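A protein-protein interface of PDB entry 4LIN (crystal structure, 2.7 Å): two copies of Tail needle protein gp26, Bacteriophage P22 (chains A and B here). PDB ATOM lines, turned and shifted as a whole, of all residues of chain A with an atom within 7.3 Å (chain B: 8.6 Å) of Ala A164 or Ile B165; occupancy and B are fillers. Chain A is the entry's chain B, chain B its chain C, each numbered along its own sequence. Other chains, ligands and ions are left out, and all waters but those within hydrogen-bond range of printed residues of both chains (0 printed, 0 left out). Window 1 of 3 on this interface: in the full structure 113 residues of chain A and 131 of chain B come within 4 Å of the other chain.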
ATOM      1  N   ILE A 158      20.030   6.545   1.349  1.00  0.00           N
ATOM      2  CA  ILE A 158      18.858   6.755   0.498  1.00  0.00           C
ATOM      3  C   ILE A 158      19.237   6.908  -0.980  1.00  0.00           C
ATOM      4  O   ILE A 158      18.609   6.307  -1.855  1.00  0.00           O
ATOM      5  CB  ILE A 158      18.022   7.967   0.965  1.00  0.00           C
ATOM      6  CG1 ILE A 158      17.311   7.650   2.280  1.00  0.00           C
ATOM      7  CG2 ILE A 158      17.000   8.353  -0.085  1.00  0.00           C
ATOM      8  CD1 ILE A 158      16.397   8.756   2.763  1.00  0.00           C
ATOM      9  N   THR A 159      20.265   7.709  -1.249  1.00  0.00           N
ATOM     10  CA  THR A 159      20.785   7.875  -2.606  1.00  0.00           C
ATOM     11  C   THR A 159      21.275   6.533  -3.149  1.00  0.00           C
ATOM     12  O   THR A 159      21.093   6.223  -4.327  1.00  0.00           O
ATOM     13  CB  THR A 159      21.924   8.919  -2.655  1.00  0.00           C
ATOM     14  OG1 THR A 159      21.407  10.212  -2.315  1.00  0.00           O
ATOM     15  CG2 THR A 159      22.550   8.981  -4.042  1.00  0.00           C
ATOM     16  N   ALA A 160      21.884   5.736  -2.277  1.00  0.00           N
ATOM     17  CA  ALA A 160      22.290   4.382  -2.630  1.00  0.00           C
ATOM     18  C   ALA A 160      21.055   3.529  -2.897  1.00  0.00           C
ATOM     19  O   ALA A 160      21.053   2.683  -3.790  1.00  0.00           O
ATOM     20  CB  ALA A 160      23.127   3.772  -1.519  1.00  0.00           C
ATOM     21  N   ASN A 161      20.003   3.762  -2.120  1.00  0.00           N
ATOM     22  CA  ASN A 161      18.762   3.020  -2.284  1.00  0.00           C
ATOM     23  C   ASN A 161      17.993   3.376  -3.551  1.00  0.00           C
ATOM     24  O   ASN A 161      17.317   2.525  -4.118  1.00  0.00           O
ATOM     25  CB  ASN A 161      17.865   3.178  -1.056  1.00  0.00           C
ATOM     26  CG  ASN A 161      18.284   2.282   0.084  1.00  0.00           C
ATOM     27  OD1 ASN A 161      19.455   1.927   0.205  1.00  0.00           O
ATOM     28  ND2 ASN A 161      17.327   1.897   0.920  1.00  0.00           N
ATOM     29  N   THR A 162      18.086   4.628  -3.986  1.00  0.00           N
ATOM     30  CA  THR A 162      17.355   5.094  -5.164  1.00  0.00           C
ATOM     31  C   THR A 162      18.160   5.026  -6.458  1.00  0.00           C
ATOM     32  O   THR A 162      17.630   5.296  -7.535  1.00  0.00           O
ATOM     33  CB  THR A 162      16.829   6.526  -4.978  1.00  0.00           C
ATOM     34  OG1 THR A 162      17.716   7.245  -4.115  1.00  0.00           O
ATOM     35  CG2 THR A 162      15.446   6.520  -4.368  1.00  0.00           C
ATOM     36  N   LYS A 163      19.445   4.703  -6.354  1.00  0.00           N
ATOM     37  CA  LYS A 163      20.217   4.361  -7.539  1.00  0.00           C
ATOM     38  C   LYS A 163      20.093   2.855  -7.728  1.00  0.00           C
ATOM     39  O   LYS A 163      20.394   2.311  -8.791  1.00  0.00           O
ATOM     40  CB  LYS A 163      21.676   4.794  -7.384  1.00  0.00           C
ATOM     41  CG  LYS A 163      22.573   4.427  -8.559  1.00  0.00           C
ATOM     42  CD  LYS A 163      23.818   5.288  -8.605  1.00  0.00           C
ATOM     43  CE  LYS A 163      24.900   4.625  -9.431  1.00  0.00           C
ATOM     44  NZ  LYS A 163      25.464   3.442  -8.726  1.00  0.00           N
ATOM     45  N   ALA A 164      19.600   2.191  -6.688  1.00  0.00           N
ATOM     46  CA  ALA A 164      19.359   0.758  -6.738  1.00  0.00           C
ATOM     47  C   ALA A 164      18.104   0.443  -7.546  1.00  0.00           C
ATOM     48  O   ALA A 164      18.138  -0.401  -8.438  1.00  0.00           O
ATOM     49  CB  ALA A 164      19.252   0.187  -5.334  1.00  0.00           C
ATOM     50  N   ILE A 165      17.005   1.127  -7.235  1.00  0.00           N
ATOM     51  CA  ILE A 165      15.731   0.881  -7.909  1.00  0.00           C
ATOM     52  C   ILE A 165      15.611   1.524  -9.293  1.00  0.00           C
ATOM     53  O   ILE A 165      14.867   1.034 -10.136  1.00  0.00           O
ATOM     54  CB  ILE A 165      14.511   1.238  -7.031  1.00  0.00           C
ATOM     55  CG1 ILE A 165      14.901   2.241  -5.950  1.00  0.00           C
ATOM     56  CG2 ILE A 165      13.923  -0.021  -6.409  1.00  0.00           C
ATOM     57  CD1 ILE A 165      13.856   2.438  -4.872  1.00  0.00           C
ATOM     58  N   THR A 166      16.324   2.623  -9.526  1.00  0.00           N
ATOM     59  CA  THR A 166      16.351   3.215 -10.862  1.00  0.00           C
ATOM     60  C   THR A 166      17.019   2.240 -11.832  1.00  0.00           C
ATOM     61  O   THR A 166      16.559   2.056 -12.958  1.00  0.00           O
ATOM     62  CB  THR A 166      17.053   4.595 -10.878  1.00  0.00           C
ATOM     63  OG1 THR A 166      16.067   5.633 -10.816  1.00  0.00           O
ATOM     64  CG2 THR A 166      17.883   4.781 -12.139  1.00  0.00           C
ATOM     65  N   ALA A 167      18.086   1.596 -11.367  1.00  0.00           N
ATOM     66  CA  ALA A 167      18.783   0.576 -12.143  1.00  0.00           C
ATOM     67  C   ALA A 167      18.094  -0.783 -12.014  1.00  0.00           C
ATOM     68  O   ALA A 167      18.331  -1.685 -12.813  1.00  0.00           O
ATOM     69  CB  ALA A 167      20.236   0.482 -11.719  1.00  0.00           C
ATOM     70  N   LEU A 168      17.253  -0.924 -10.995  1.00  0.00           N
ATOM     71  CA  LEU A 168      16.381  -2.084 -10.889  1.00  0.00           C
ATOM     72  C   LEU A 168      15.250  -1.913 -11.898  1.00  0.00           C
ATOM     73  O   LEU A 168      14.751  -2.892 -12.453  1.00  0.00           O
ATOM     74  CB  LEU A 168      15.809  -2.216  -9.474  1.00  0.00           C
ATOM     75  CG  LEU A 168      16.192  -3.396  -8.576  1.00  0.00           C
ATOM     76  CD1 LEU A 168      17.700  -3.559  -8.460  1.00  0.00           C
ATOM     77  CD2 LEU A 168      15.574  -3.222  -7.195  1.00  0.00           C
ATOM     78  N   ASN A 169      14.843  -0.667 -12.128  1.00  0.00           N
ATOM     79  CA  ASN A 169      13.775  -0.366 -13.083  1.00  0.00           C
ATOM     80  C   ASN A 169      14.198  -0.521 -14.539  1.00  0.00           C
ATOM     81  O   ASN A 169      13.394  -0.899 -15.389  1.00  0.00           O
ATOM     82  CB  ASN A 169      13.227   1.050 -12.852  1.00  0.00           C
ATOM     83  CG  ASN A 169      12.083   1.084 -11.863  1.00  0.00           C
ATOM     84  OD1 ASN A 169      12.276   0.901 -10.667  1.00  0.00           O
ATOM     85  ND2 ASN A 169      10.880   1.331 -12.362  1.00  0.00           N
ATOM     86  N   VAL A 170      15.460  -0.210 -14.821  1.00  0.00           N
ATOM     87  CA  VAL A 170      15.980  -0.308 -16.178  1.00  0.00           C
ATOM     88  C   VAL A 170      16.134  -1.776 -16.581  1.00  0.00           C
ATOM     89  O   VAL A 170      16.045  -2.115 -17.759  1.00  0.00           O
ATOM     90  CB  VAL A 170      17.323   0.459 -16.338  1.00  0.00           C
ATOM     91  CG1 VAL A 170      18.447  -0.258 -15.619  1.00  0.00           C
ATOM     92  CG2 VAL A 170      17.674   0.646 -17.796  1.00  0.00           C
ATOM     93  N   ILE B 158      14.786   2.339   6.001  1.00  0.00           N
ATOM     94  CA  ILE B 158      15.845   2.261   4.991  1.00  0.00           C
ATOM     95  C   ILE B 158      16.405   0.846   4.907  1.00  0.00           C
ATOM     96  O   ILE B 158      16.585   0.300   3.815  1.00  0.00           O
ATOM     97  CB  ILE B 158      17.035   3.192   5.347  1.00  0.00           C
ATOM     98  CG1 ILE B 158      16.668   4.663   5.174  1.00  0.00           C
ATOM     99  CG2 ILE B 158      18.255   2.867   4.497  1.00  0.00           C
ATOM    100  CD1 ILE B 158      17.853   5.605   5.279  1.00  0.00           C
ATOM    101  N   THR B 159      16.663   0.253   6.069  1.00  0.00           N
ATOM    102  CA  THR B 159      17.249  -1.080   6.141  1.00  0.00           C
ATOM    103  C   THR B 159      16.304  -2.172   5.623  1.00  0.00           C
ATOM    104  O   THR B 159      16.755  -3.165   5.052  1.00  0.00           O
ATOM    105  CB  THR B 159      17.761  -1.400   7.574  1.00  0.00           C
ATOM    106  OG1 THR B 159      19.016  -2.086   7.499  1.00  0.00           O
ATOM    107  CG2 THR B 159      16.761  -2.242   8.359  1.00  0.00           C
ATOM    108  N   ALA B 160      15.000  -1.981   5.805  1.00  0.00           N
ATOM    109  CA  ALA B 160      14.021  -2.920   5.274  1.00  0.00           C
ATOM    110  C   ALA B 160      13.892  -2.710   3.771  1.00  0.00           C
ATOM    111  O   ALA B 160      13.565  -3.638   3.030  1.00  0.00           O
ATOM    112  CB  ALA B 160      12.678  -2.748   5.963  1.00  0.00           C
ATOM    113  N   ASN B 161      14.149  -1.483   3.329  1.00  0.00           N
ATOM    114  CA  ASN B 161      14.170  -1.165   1.908  1.00  0.00           C
ATOM    115  C   ASN B 161      15.368  -1.798   1.205  1.00  0.00           C
ATOM    116  O   ASN B 161      15.242  -2.330   0.106  1.00  0.00           O
ATOM    117  CB  ASN B 161      14.176   0.351   1.693  1.00  0.00           C
ATOM    118  CG  ASN B 161      12.859   1.001   2.064  1.00  0.00           C
ATOM    119  OD1 ASN B 161      12.001   0.376   2.683  1.00  0.00           O
ATOM    120  ND2 ASN B 161      12.693   2.262   1.684  1.00  0.00           N
ATOM    121  N   THR B 162      16.528  -1.732   1.853  1.00  0.00           N
ATOM    122  CA  THR B 162      17.759  -2.304   1.314  1.00  0.00           C
ATOM    123  C   THR B 162      17.697  -3.824   1.266  1.00  0.00           C
ATOM    124  O   THR B 162      18.301  -4.457   0.404  1.00  0.00           O
ATOM    125  CB  THR B 162      18.977  -1.916   2.175  1.00  0.00           C
ATOM    126  OG1 THR B 162      18.732  -2.286   3.537  1.00  0.00           O
ATOM    127  CG2 THR B 162      19.227  -0.434   2.114  1.00  0.00           C
ATOM    128  N   LYS B 163      16.968  -4.399   2.214  1.00  0.00           N
ATOM    129  CA  LYS B 163      16.900  -5.844   2.379  1.00  0.00           C
ATOM    130  C   LYS B 163      16.012  -6.480   1.316  1.00  0.00           C
ATOM    131  O   LYS B 163      16.280  -7.588   0.855  1.00  0.00           O
ATOM    132  CB  LYS B 163      16.366  -6.174   3.773  1.00  0.00           C
ATOM    133  CG  LYS B 163      16.589  -7.602   4.227  1.00  0.00           C
ATOM    134  CD  LYS B 163      15.772  -7.870   5.479  1.00  0.00           C
ATOM    135  CE  LYS B 163      16.239  -9.110   6.213  1.00  0.00           C
ATOM    136  NZ  LYS B 163      15.511  -9.261   7.502  1.00  0.00           N
ATOM    137  N   ALA B 164      14.947  -5.780   0.939  1.00  0.00           N
ATOM    138  CA  ALA B 164      14.041  -6.272  -0.090  1.00  0.00           C
ATOM    139  C   ALA B 164      14.472  -5.836  -1.490  1.00  0.00           C
ATOM    140  O   ALA B 164      13.939  -6.322  -2.486  1.00  0.00           O
ATOM    141  CB  ALA B 164      12.611  -5.844   0.200  1.00  0.00           C
ATOM    142  N   ILE B 165      15.428  -4.911  -1.557  1.00  0.00           N
ATOM    143  CA  ILE B 165      16.055  -4.553  -2.828  1.00  0.00           C
ATOM    144  C   ILE B 165      17.023  -5.662  -3.223  1.00  0.00           C
ATOM    145  O   ILE B 165      17.062  -6.093  -4.375  1.00  0.00           O
ATOM    146  CB  ILE B 165      16.790  -3.192  -2.752  1.00  0.00           C
ATOM    147  CG1 ILE B 165      15.815  -2.052  -3.036  1.00  0.00           C
ATOM    148  CG2 ILE B 165      17.946  -3.135  -3.740  1.00  0.00           C
ATOM    149  CD1 ILE B 165      16.468  -0.700  -3.217  1.00  0.00           C
ATOM    150  N   THR B 166      17.792  -6.125  -2.245  1.00  0.00           N
ATOM    151  CA  THR B 166      18.684  -7.260  -2.423  1.00  0.00           C
ATOM    152  C   THR B 166      17.896  -8.528  -2.746  1.00  0.00           C
ATOM    153  O   THR B 166      18.338  -9.357  -3.537  1.00  0.00           O
ATOM    154  CB  THR B 166      19.530  -7.500  -1.159  1.00  0.00           C
ATOM    155  OG1 THR B 166      18.679  -7.485  -0.006  1.00  0.00           O
ATOM    156  CG2 THR B 166      20.584  -6.415  -1.009  1.00  0.00           C
ATOM    157  N   ALA B 167      16.724  -8.665  -2.135  1.00  0.00           N
ATOM    158  CA  ALA B 167      15.905  -9.863  -2.301  1.00  0.00           C
ATOM    159  C   ALA B 167      15.210  -9.928  -3.660  1.00  0.00           C
ATOM    160  O   ALA B 167      14.930 -11.016  -4.162  1.00  0.00           O
ATOM    161  CB  ALA B 167      14.883  -9.972  -1.177  1.00  0.00           C
ATOM    162  N   LEU B 168      14.898  -8.773  -4.239  1.00  0.00           N
ATOM    163  CA  LEU B 168      14.308  -8.758  -5.573  1.00  0.00           C
ATOM    164  C   LEU B 168      15.366  -8.661  -6.676  1.00  0.00           C
ATOM    165  O   LEU B 168      15.068  -8.896  -7.843  1.00  0.00           O
ATOM    166  CB  LEU B 168      13.256  -7.645  -5.699  1.00  0.00           C
ATOM    167  CG  LEU B 168      13.669  -6.238  -6.135  1.00  0.00           C
ATOM    168  CD1 LEU B 168      13.492  -6.067  -7.634  1.00  0.00           C
ATOM    169  CD2 LEU B 168      12.866  -5.189  -5.385  1.00  0.00           C
ATOM    170  N   ASN B 169      16.598  -8.332  -6.301  1.00  0.00           N
ATOM    171  CA  ASN B 169      17.698  -8.294  -7.257  1.00  0.00           C
ATOM    172  C   ASN B 169      18.197  -9.701  -7.549  1.00  0.00           C
ATOM    173  O   ASN B 169      18.653 -10.000  -8.655  1.00  0.00           O
ATOM    174  CB  ASN B 169      18.843  -7.420  -6.737  1.00  0.00           C
ATOM    175  CG  ASN B 169      20.107  -7.550  -7.574  1.00  0.00           C
ATOM    176  OD1 ASN B 169      20.925  -8.441  -7.348  1.00  0.00           O
ATOM    177  ND2 ASN B 169      20.274  -6.654  -8.539  1.00  0.00           N
ATOM    178  N   VAL B 170      18.106 -10.562  -6.541  1.00  0.00           N
ATOM    179  CA  VAL B 170      18.498 -11.955  -6.695  1.00  0.00           C
ATOM    180  C   VAL B 170      17.391 -12.752  -7.376  1.00  0.00           C
ATOM    181  O   VAL B 170      17.615 -13.881  -7.815  1.00  0.00           O
ATOM    182  CB  VAL B 170      18.889 -12.596  -5.344  1.00  0.00           C
ATOM    183  CG1 VAL B 170      20.179 -11.984  -4.825  1.00  0.00           C
ATOM    184  CG2 VAL B 170      17.771 -12.431  -4.329  1.00  0.00           C
ATOM    185  N   ARG B 171      16.187 -12.192  -7.420  1.00  0.00           N
ATOM    186  CA  ARG B 171      15.140 -12.726  -8.282  1.00  0.00           C
ATOM    187  C   ARG B 171      15.189 -12.158  -9.705  1.00  0.00           C
ATOM    188  O   ARG B 171      14.654 -12.760 -10.633  1.00  0.00           O
ATOM    189  CB  ARG B 171      13.757 -12.503  -7.678  1.00  0.00           C
ATOM    190  CG  ARG B 171      13.516 -13.172  -6.336  1.00  0.00           C
ATOM    191  CD  ARG B 171      12.023 -13.267  -6.070  1.00  0.00           C
ATOM    192  NE  ARG B 171      11.339 -12.043  -6.477  1.00  0.00           N
ATOM    193  CZ  ARG B 171      10.020 -11.904  -6.550  1.00  0.00           C
ATOM    194  NH1 ARG B 171       9.222 -12.917  -6.243  1.00  0.00           N
ATOM    195  NH2 ARG B 171       9.495 -10.749  -6.935  1.00  0.00           N
ATOM    196  N   VAL B 172      15.797 -10.982  -9.876  1.00  0.00           N
ATOM    197  CA  VAL B 172      15.912 -10.387 -11.211  1.00  0.00           C
ATOM    198  C   VAL B 172      17.091 -10.933 -12.011  1.00  0.00           C
ATOM    199  O   VAL B 172      16.953 -11.255 -13.192  1.00  0.00           O
ATOM    200  CB  VAL B 172      15.953  -8.841 -11.175  1.00  0.00           C
ATOM    201  CG1 VAL B 172      16.412  -8.282 -12.510  1.00  0.00           C
ATOM    202  CG2 VAL B 172      14.590  -8.293 -10.843  1.00  0.00           C
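The side-chain amide nitrogen of Asn A161 sits at hydrogen-bond distance from the backbone carbonyl oxygen of Ile B158.
O of Ile A158 is in hydrogen-bond range of OG1 of Thr A162 (2.6 Å).
The backbone carbonyl oxygen (O) of Ile B158 sits close to the side-chain hydroxyl (OG1) of Thr B162.
OG1 of Thr B162 lies within hydrogen-bond range of O of Thr B159.
OG1 of Thr B166 sits at hydrogen-bond distance from O of Thr B162 (3.1 Å).
Among the printed residues, pairs that only touch across the chains: Asn A161 with Thr B162 (3.0 Å), Asn A161 with Ile B165 (3.5 Å), Leu A168 with Leu B168 (3.6 Å), Asn A161 with Asn B161 (3.6 Å), Ala A164 with Ile B165 (3.6 Å) and Ile A158 with Ile B158 (3.7 Å).
Ala A164 touches one residue of chain B.
Of the printed residues of chain A, Asn B161 touches Asn A161 (3.6 Å).
Printed residues of chain A within 4 Å of Thr B162: Asn A161 (3.0 Å).
Ile B165 touches just these residues of chain A: Asn A161 and Ala A164.
The nearest residue of chain B that does not touch Ala A164 is Asn B169 (6.6 Å).
The nearest residue of chain A that does not touch Ile B165 is Ile A165 (4.1 Å).
Hydrophobic or aromatic side chains of chain A that line the printed part of chain B: Ile A158, Ala A164 and Leu A168.
Hydrophobic or aromatic side chains of chain B that line the printed part of chain A: Ile B158, Ile B165 and Leu B168.
Asn A161 touches Ile B158, but with the chains exchanged Ile A158 does not touch Asn B161 (7.1 Å).
Asn A161 touches Ile B165, but with the chains exchanged Ile A165 does not touch Asn B161 (6.7 Å).
Ala A164 touches Ile B165, but with the chains exchanged Ile A165 does not touch Ala B164 (7.4 Å).
Leu B168 touches its own counterpart, Leu A168.
Positions printed for both chains: 158, 159, 160, 161, 162, 163, 164, 165, 166, 167, 168, 169 and 170.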
